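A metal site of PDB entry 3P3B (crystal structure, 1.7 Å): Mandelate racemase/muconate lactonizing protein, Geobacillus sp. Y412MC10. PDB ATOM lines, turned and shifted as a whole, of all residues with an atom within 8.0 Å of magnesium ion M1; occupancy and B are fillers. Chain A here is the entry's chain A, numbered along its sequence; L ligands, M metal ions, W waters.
The side-chain carboxylate of Glu 233 sits at hydrogen-bond distance from the side-chain amide nitrogen of Gln 283 (2.9 Å).
The backbone carbonyl oxygen (O) of Glu 233 sits at hydrogen-bond distance from the backbone NH (N) of Ala 208 (3.1 Å).
The backbone NH (N) of Glu 233 lies within hydrogen-bond range of the backbone carbonyl oxygen (O) of Ile 206 (2.8 Å).
The side-chain amino group (NZ) of Lys 168 lies close to the side-chain carboxylate (OD2) of Asp 207, at 3.8 Å.
The backbone NH (N) of Asn 209 lies within hydrogen-bond range of the side-chain carboxylate (OD1) of Asp 207.
OD2 of Asp 207 lies close to NZ of Lys 170 (3.1 Å).
NZ of Lys 168 lies within salt-bridge range of OE2 of Glu 336 (3.3 Å).
NZ of Lys 168 is in hydrogen-bond range of OH of Tyr 131, at 2.8 Å.
Lys 168 touches magnesium ion M1 (NZ to MG, 3.8 Å).
Of the 24 residues printed, 4 come within 4 Å of magnesium ion M1.
Magnesium ion M1 is bound by the side-chain carboxylate (OE2) of Glu 233 (2.1 Å).
An oxygen (O2) of the ligand is bound to magnesium ion M1, 2.1 Å away.
OD2 of Asp 207 binds magnesium ion M1 (2.2 Å).
Water W1 binds magnesium ion M1 (2.2 Å).
Magnesium ion M1 is bound by OE2 of Glu 263 (2.2 Å).
O3 of the ligand is bound to magnesium ion M1.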
ATOM      1  N   ASN A  33     -14.015 -22.347  -4.419  1.00  0.00           N
ATOM      2  CA  ASN A  33     -13.685 -21.307  -3.446  1.00  0.00           C
ATOM      3  C   ASN A  33     -13.225 -20.062  -4.198  1.00  0.00           C
ATOM      4  O   ASN A  33     -13.320 -20.004  -5.418  1.00  0.00           O
ATOM      5  CB  ASN A  33     -12.625 -21.769  -2.424  1.00  0.00           C
ATOM      6  CG  ASN A  33     -11.257 -22.024  -3.032  1.00  0.00           C
ATOM      7  OD1 ASN A  33     -10.964 -21.622  -4.156  1.00  0.00           O
ATOM      8  ND2 ASN A  33     -10.418 -22.714  -2.270  1.00  0.00           N
ATOM      9  N   TYR A 131     -15.120 -26.886  14.055  1.00  0.00           N
ATOM     10  CA  TYR A 131     -16.005 -26.134  13.178  1.00  0.00           C
ATOM     11  C   TYR A 131     -16.219 -26.876  11.862  1.00  0.00           C
ATOM     12  O   TYR A 131     -15.378 -27.660  11.416  1.00  0.00           O
ATOM     13  CB  TYR A 131     -15.525 -24.694  12.936  1.00  0.00           C
ATOM     14  CG  TYR A 131     -14.249 -24.560  12.113  1.00  0.00           C
ATOM     15  CD1 TYR A 131     -14.295 -24.617  10.710  1.00  0.00           C
ATOM     16  CD2 TYR A 131     -13.014 -24.342  12.720  1.00  0.00           C
ATOM     17  CE1 TYR A 131     -13.132 -24.505   9.942  1.00  0.00           C
ATOM     18  CE2 TYR A 131     -11.840 -24.216  11.969  1.00  0.00           C
ATOM     19  CZ  TYR A 131     -11.918 -24.293  10.586  1.00  0.00           C
ATOM     20  OH  TYR A 131     -10.788 -24.159   9.834  1.00  0.00           O
ATOM     21  N   THR A 133     -16.246 -26.897   8.136  1.00  0.00           N
ATOM     22  CA  THR A 133     -15.531 -26.173   7.091  1.00  0.00           C
ATOM     23  C   THR A 133     -16.125 -26.341   5.698  1.00  0.00           C
ATOM     24  O   THR A 133     -15.555 -25.864   4.700  1.00  0.00           O
ATOM     25  CB  THR A 133     -14.032 -26.598   7.092  1.00  0.00           C
ATOM     26  OG1 THR A 133     -13.232 -25.599   6.436  1.00  0.00           O
ATOM     27  CG2 THR A 133     -13.815 -27.963   6.412  1.00  0.00           C
ATOM     28  N   TYR A 136     -18.774 -24.229   0.969  1.00  0.00           N
ATOM     29  CA  TYR A 136     -18.070 -23.748  -0.224  1.00  0.00           C
ATOM     30  C   TYR A 136     -19.021 -22.899  -1.088  1.00  0.00           C
ATOM     31  O   TYR A 136     -20.101 -22.557  -0.620  1.00  0.00           O
ATOM     32  CB  TYR A 136     -17.433 -24.943  -0.969  1.00  0.00           C
ATOM     33  CG  TYR A 136     -16.062 -25.262  -0.378  1.00  0.00           C
ATOM     34  CD1 TYR A 136     -15.954 -25.823   0.891  1.00  0.00           C
ATOM     35  CD2 TYR A 136     -14.891 -24.952  -1.066  1.00  0.00           C
ATOM     36  CE1 TYR A 136     -14.684 -26.074   1.461  1.00  0.00           C
ATOM     37  CE2 TYR A 136     -13.630 -25.193  -0.492  1.00  0.00           C
ATOM     38  CZ  TYR A 136     -13.543 -25.763   0.756  1.00  0.00           C
ATOM     39  OH  TYR A 136     -12.280 -25.973   1.312  1.00  0.00           O
ATOM     40  N   LYS A 168     -17.364 -22.265   9.140  1.00  0.00           N
ATOM     41  CA  LYS A 168     -16.466 -21.446   8.360  1.00  0.00           C
ATOM     42  C   LYS A 168     -17.035 -21.354   6.954  1.00  0.00           C
ATOM     43  O   LYS A 168     -17.226 -22.363   6.265  1.00  0.00           O
ATOM     44  CB  LYS A 168     -15.016 -21.976   8.347  1.00  0.00           C
ATOM     45  CG  LYS A 168     -14.041 -21.013   7.621  1.00  0.00           C
ATOM     46  CD  LYS A 168     -12.571 -21.296   7.945  1.00  0.00           C
ATOM     47  CE  LYS A 168     -11.956 -22.323   6.951  1.00  0.00           C
ATOM     48  NZ  LYS A 168     -10.601 -22.792   7.407  1.00  0.00           N
ATOM     49  N   LYS A 170     -16.887 -20.007   3.102  1.00  0.00           N
ATOM     50  CA  LYS A 170     -16.083 -19.496   1.988  1.00  0.00           C
ATOM     51  C   LYS A 170     -16.686 -18.200   1.447  1.00  0.00           C
ATOM     52  O   LYS A 170     -17.885 -18.144   1.150  1.00  0.00           O
ATOM     53  CB  LYS A 170     -15.956 -20.531   0.868  1.00  0.00           C
ATOM     54  CG  LYS A 170     -15.057 -21.765   1.202  1.00  0.00           C
ATOM     55  CD  LYS A 170     -13.629 -21.331   1.423  1.00  0.00           C
ATOM     56  CE  LYS A 170     -12.689 -22.460   1.842  1.00  0.00           C
ATOM     57  NZ  LYS A 170     -12.677 -22.627   3.317  1.00  0.00           N
ATOM     58  N   ILE A 206     -14.923 -16.617   8.332  1.00  0.00           N
ATOM     59  CA  ILE A 206     -14.989 -16.404   6.892  1.00  0.00           C
ATOM     60  C   ILE A 206     -13.624 -16.539   6.246  1.00  0.00           C
ATOM     61  O   ILE A 206     -12.641 -16.082   6.799  1.00  0.00           O
ATOM     62  CB  ILE A 206     -15.650 -15.058   6.500  1.00  0.00           C
ATOM     63  CG1 ILE A 206     -14.837 -13.859   6.988  1.00  0.00           C
ATOM     64  CG2 ILE A 206     -17.131 -15.037   6.950  1.00  0.00           C
ATOM     65  CD1 ILE A 206     -15.406 -12.519   6.425  1.00  0.00           C
ATOM     66  N   ASP A 207     -13.586 -17.183   5.085  1.00  0.00           N
ATOM     67  CA  ASP A 207     -12.314 -17.527   4.447  1.00  0.00           C
ATOM     68  C   ASP A 207     -12.385 -17.084   2.995  1.00  0.00           C
ATOM     69  O   ASP A 207     -13.189 -17.615   2.218  1.00  0.00           O
ATOM     70  CB  ASP A 207     -12.069 -19.038   4.593  1.00  0.00           C
ATOM     71  CG  ASP A 207     -10.744 -19.504   4.014  1.00  0.00           C
ATOM     72  OD1 ASP A 207     -10.054 -18.732   3.303  1.00  0.00           O
ATOM     73  OD2 ASP A 207     -10.404 -20.686   4.256  1.00  0.00           O
ATOM     74  N   ALA A 208     -11.567 -16.104   2.637  1.00  0.00           N
ATOM     75  CA  ALA A 208     -11.628 -15.512   1.308  1.00  0.00           C
ATOM     76  C   ALA A 208     -10.719 -16.191   0.300  1.00  0.00           C
ATOM     77  O   ALA A 208     -10.789 -15.881  -0.893  1.00  0.00           O
ATOM     78  CB  ALA A 208     -11.295 -13.991   1.385  1.00  0.00           C
ATOM     79  N   ASN A 209      -9.875 -17.113   0.766  1.00  0.00           N
ATOM     80  CA  ASN A 209      -8.856 -17.712  -0.097  1.00  0.00           C
ATOM     81  C   ASN A 209      -8.113 -16.695  -0.973  1.00  0.00           C
ATOM     82  O   ASN A 209      -7.932 -16.886  -2.177  1.00  0.00           O
ATOM     83  CB  ASN A 209      -9.436 -18.885  -0.908  1.00  0.00           C
ATOM     84  CG  ASN A 209      -9.815 -20.048  -0.029  1.00  0.00           C
ATOM     85  OD1 ASN A 209     -10.969 -20.197   0.349  1.00  0.00           O
ATOM     86  ND2 ASN A 209      -8.827 -20.857   0.343  1.00  0.00           N
ATOM     87  N   ASN A 210      -7.722 -15.601  -0.319  1.00  0.00           N
ATOM     88  CA  ASN A 210      -6.921 -14.519  -0.885  1.00  0.00           C
ATOM     89  C   ASN A 210      -7.577 -13.671  -1.975  1.00  0.00           C
ATOM     90  O   ASN A 210      -6.889 -12.897  -2.629  1.00  0.00           O
ATOM     91  CB  ASN A 210      -5.545 -15.029  -1.335  1.00  0.00           C
ATOM     92  CG  ASN A 210      -4.653 -15.364  -0.156  1.00  0.00           C
ATOM     93  OD1 ASN A 210      -4.855 -14.859   0.958  1.00  0.00           O
ATOM     94  ND2 ASN A 210      -3.644 -16.212  -0.384  1.00  0.00           N
ATOM     95  N   TRP A 231     -13.346 -15.161  13.257  1.00  0.00           N
ATOM     96  CA  TRP A 231     -12.110 -14.817  12.547  1.00  0.00           C
ATOM     97  C   TRP A 231     -12.268 -14.639  11.055  1.00  0.00           C
ATOM     98  O   TRP A 231     -13.248 -15.110  10.452  1.00  0.00           O
ATOM     99  CB  TRP A 231     -10.943 -15.780  12.863  1.00  0.00           C
ATOM    100  CG  TRP A 231     -10.863 -17.142  12.136  1.00  0.00           C
ATOM    101  CD1 TRP A 231     -11.003 -17.411  10.791  1.00  0.00           C
ATOM    102  CD2 TRP A 231     -10.527 -18.381  12.756  1.00  0.00           C
ATOM    103  NE1 TRP A 231     -10.803 -18.775  10.556  1.00  0.00           N
ATOM    104  CE2 TRP A 231     -10.519 -19.376  11.747  1.00  0.00           C
ATOM    105  CE3 TRP A 231     -10.267 -18.747  14.083  1.00  0.00           C
ATOM    106  CZ2 TRP A 231     -10.241 -20.716  12.042  1.00  0.00           C
ATOM    107  CZ3 TRP A 231      -9.982 -20.085  14.366  1.00  0.00           C
ATOM    108  CH2 TRP A 231      -9.973 -21.049  13.338  1.00  0.00           C
ATOM    109  N   GLU A 233     -10.112 -15.234   7.642  1.00  0.00           N
ATOM    110  CA  GLU A 233      -9.023 -16.101   7.202  1.00  0.00           C
ATOM    111  C   GLU A 233      -8.623 -15.801   5.767  1.00  0.00           C
ATOM    112  O   GLU A 233      -9.483 -15.747   4.871  1.00  0.00           O
ATOM    113  CB  GLU A 233      -9.454 -17.562   7.369  1.00  0.00           C
ATOM    114  CG  GLU A 233      -8.531 -18.576   6.698  1.00  0.00           C
ATOM    115  CD  GLU A 233      -8.839 -19.994   7.118  1.00  0.00           C
ATOM    116  OE1 GLU A 233      -9.566 -20.210   8.122  1.00  0.00           O
ATOM    117  OE2 GLU A 233      -8.320 -20.912   6.470  1.00  0.00           O
ATOM    118  N   GLU A 234      -7.322 -15.607   5.548  1.00  0.00           N
ATOM    119  CA  GLU A 234      -6.773 -15.339   4.202  1.00  0.00           C
ATOM    120  C   GLU A 234      -7.591 -14.334   3.393  1.00  0.00           C
ATOM    121  O   GLU A 234      -8.059 -14.610   2.286  1.00  0.00           O
ATOM    122  CB  GLU A 234      -6.573 -16.650   3.438  1.00  0.00           C
ATOM    123  CG  GLU A 234      -5.511 -17.558   4.083  1.00  0.00           C
ATOM    124  CD  GLU A 234      -4.783 -18.441   3.066  1.00  0.00           C
ATOM    125  OE1 GLU A 234      -5.427 -19.294   2.416  1.00  0.00           O
ATOM    126  OE2 GLU A 234      -3.547 -18.290   2.959  1.00  0.00           O
ATOM    127  N   ALA A 260      -6.628 -14.625  10.843  1.00  0.00           N
ATOM    128  CA  ALA A 260      -6.096 -15.994  10.709  1.00  0.00           C
ATOM    129  C   ALA A 260      -5.397 -16.191   9.351  1.00  0.00           C
ATOM    130  O   ALA A 260      -5.886 -15.730   8.322  1.00  0.00           O
ATOM    131  CB  ALA A 260      -7.250 -17.010  10.850  1.00  0.00           C
ATOM    132  N   ASP A 261      -4.247 -16.844   9.356  1.00  0.00           N
ATOM    133  CA  ASP A 261      -3.496 -17.060   8.124  1.00  0.00           C
ATOM    134  C   ASP A 261      -2.480 -18.192   8.355  1.00  0.00           C
ATOM    135  O   ASP A 261      -2.292 -18.640   9.485  1.00  0.00           O
ATOM    136  CB  ASP A 261      -2.809 -15.753   7.664  1.00  0.00           C
ATOM    137  CG  ASP A 261      -2.828 -15.615   6.147  1.00  0.00           C
ATOM    138  OD1 ASP A 261      -2.637 -16.655   5.476  1.00  0.00           O
ATOM    139  OD2 ASP A 261      -3.054 -14.500   5.619  1.00  0.00           O
ATOM    140  N   GLY A 262      -1.855 -18.644   7.272  1.00  0.00           N
ATOM    141  CA  GLY A 262      -0.724 -19.556   7.385  1.00  0.00           C
ATOM    142  C   GLY A 262      -0.815 -20.856   6.595  1.00  0.00           C
ATOM    143  O   GLY A 262       0.180 -21.587   6.530  1.00  0.00           O
ATOM    144  N   GLU A 263      -1.961 -21.156   5.992  1.00  0.00           N
ATOM    145  CA  GLU A 263      -1.998 -22.367   5.167  1.00  0.00           C
ATOM    146  C   GLU A 263      -1.230 -22.178   3.843  1.00  0.00           C
ATOM    147  O   GLU A 263      -0.850 -21.072   3.483  1.00  0.00           O
ATOM    148  CB  GLU A 263      -3.435 -22.794   4.893  1.00  0.00           C
ATOM    149  CG  GLU A 263      -4.089 -22.020   3.766  1.00  0.00           C
ATOM    150  CD  GLU A 263      -5.560 -22.297   3.631  1.00  0.00           C
ATOM    151  OE1 GLU A 263      -5.967 -22.762   2.542  1.00  0.00           O
ATOM    152  OE2 GLU A 263      -6.309 -22.067   4.619  1.00  0.00           O
ATOM    153  N   GLY A 264      -1.010 -23.279   3.120  1.00  0.00           N
ATOM    154  CA  GLY A 264      -0.382 -23.216   1.816  1.00  0.00           C
ATOM    155  C   GLY A 264       1.058 -22.715   1.833  1.00  0.00           C
ATOM    156  O   GLY A 264       1.806 -22.956   2.778  1.00  0.00           O
ATOM    157  N   GLN A 283      -2.150 -21.054  10.948  1.00  0.00           N
ATOM    158  CA  GLN A 283      -2.899 -22.168  10.347  1.00  0.00           C
ATOM    159  C   GLN A 283      -2.059 -23.111   9.467  1.00  0.00           C
ATOM    160  O   GLN A 283      -2.526 -23.640   8.455  1.00  0.00           O
ATOM    161  CB  GLN A 283      -4.101 -21.608   9.575  1.00  0.00           C
ATOM    162  CG  GLN A 283      -5.072 -20.834  10.457  1.00  0.00           C
ATOM    163  CD  GLN A 283      -6.254 -20.291   9.651  1.00  0.00           C
ATOM    164  OE1 GLN A 283      -6.076 -19.602   8.653  1.00  0.00           O
ATOM    165  NE2 GLN A 283      -7.470 -20.605  10.097  1.00  0.00           N
ATOM    166  N   HIS A 311      -4.489 -26.045   9.856  1.00  0.00           N
ATOM    167  CA  HIS A 311      -5.277 -26.271   8.647  1.00  0.00           C
ATOM    168  C   HIS A 311      -5.453 -27.766   8.377  1.00  0.00           C
ATOM    169  O   HIS A 311      -4.531 -28.586   8.592  1.00  0.00           O
ATOM    170  CB  HIS A 311      -4.597 -25.604   7.431  1.00  0.00           C
ATOM    171  CG  HIS A 311      -5.179 -26.005   6.111  1.00  0.00           C
ATOM    172  ND1 HIS A 311      -4.899 -27.200   5.490  1.00  0.00           N
ATOM    173  CD2 HIS A 311      -6.040 -25.345   5.282  1.00  0.00           C
ATOM    174  CE1 HIS A 311      -5.540 -27.267   4.335  1.00  0.00           C
ATOM    175  NE2 HIS A 311      -6.245 -26.145   4.192  1.00  0.00           N
ATOM    176  N   CYS A 312      -6.638 -28.136   7.928  1.00  0.00           N
ATOM    177  CA  CYS A 312      -6.843 -29.508   7.473  1.00  0.00           C
ATOM    178  C   CYS A 312      -7.948 -29.480   6.438  1.00  0.00           C
ATOM    179  O   CYS A 312      -9.082 -29.069   6.713  1.00  0.00           O
ATOM    180  CB  CYS A 312      -7.246 -30.448   8.602  1.00  0.00           C
ATOM    181  SG  CYS A 312      -7.495 -32.186   8.056  1.00  0.00           S
ATOM    182  N   TYR A 313      -7.588 -29.869   5.229  1.00  0.00           N
ATOM    183  CA  TYR A 313      -8.578 -30.004   4.158  1.00  0.00           C
ATOM    184  C   TYR A 313      -7.954 -30.828   3.066  1.00  0.00           C
ATOM    185  O   TYR A 313      -6.778 -30.646   2.706  1.00  0.00           O
ATOM    186  CB  TYR A 313      -9.013 -28.647   3.593  1.00  0.00           C
ATOM    187  CG  TYR A 313     -10.291 -28.781   2.785  1.00  0.00           C
ATOM    188  CD1 TYR A 313     -11.521 -28.841   3.417  1.00  0.00           C
ATOM    189  CD2 TYR A 313     -10.254 -28.856   1.395  1.00  0.00           C
ATOM    190  CE1 TYR A 313     -12.723 -28.998   2.682  1.00  0.00           C
ATOM    191  CE2 TYR A 313     -11.442 -29.009   0.636  1.00  0.00           C
ATOM    192  CZ  TYR A 313     -12.670 -29.076   1.284  1.00  0.00           C
ATOM    193  OH  TYR A 313     -13.844 -29.234   0.566  1.00  0.00           O
ATOM    194  N   GLU A 336     -10.518 -28.373  12.383  1.00  0.00           N
ATOM    195  CA  GLU A 336     -11.218 -28.023  11.154  1.00  0.00           C
ATOM    196  C   GLU A 336     -11.892 -29.292  10.635  1.00  0.00           C
ATOM    197  O   GLU A 336     -11.211 -30.208  10.163  1.00  0.00           O
ATOM    198  CB  GLU A 336     -10.249 -27.510  10.087  1.00  0.00           C
ATOM    199  CG  GLU A 336     -10.926 -27.184   8.734  1.00  0.00           C
ATOM    200  CD  GLU A 336     -10.042 -26.417   7.771  1.00  0.00           C
ATOM    201  OE1 GLU A 336      -8.845 -26.195   8.051  1.00  0.00           O
ATOM    202  OE2 GLU A 336     -10.566 -25.993   6.723  1.00  0.00           O
HETATM  203  O1  LIG L   1      -9.459 -25.488   4.619  1.00  0.00           O
HETATM  204  O2  LIG L   1      -9.115 -23.411   5.172  1.00  0.00           O
HETATM  205  C1  LIG L   1      -9.302 -24.284   4.295  1.00  0.00           C
HETATM  206  C2  LIG L   1      -9.368 -23.899   2.845  1.00  0.00           C
HETATM  207  O3  LIG L   1      -8.504 -22.792   2.510  1.00  0.00           O
HETATM  208  C3  LIG L   1      -9.020 -25.038   1.892  1.00  0.00           C
HETATM  209  O4  LIG L   1      -7.638 -25.401   2.026  1.00  0.00           O
HETATM  210  C4  LIG L   1      -9.301 -24.665   0.463  1.00  0.00           C
HETATM  211  O5  LIG L   1     -10.502 -24.460   0.133  1.00  0.00           O
HETATM  212  O6  LIG L   1      -8.314 -24.572  -0.321  1.00  0.00           O
HETATM  213 MG    MG M   1      -8.426 -21.513   4.505  1.00  0.00          MG
HETATM  214 MG    MG M   2      -2.055 -16.853   3.462  1.00  0.00          MG
HETATM  215  O   HOH W   1      -7.649 -19.881   3.304  1.00  0.00           O
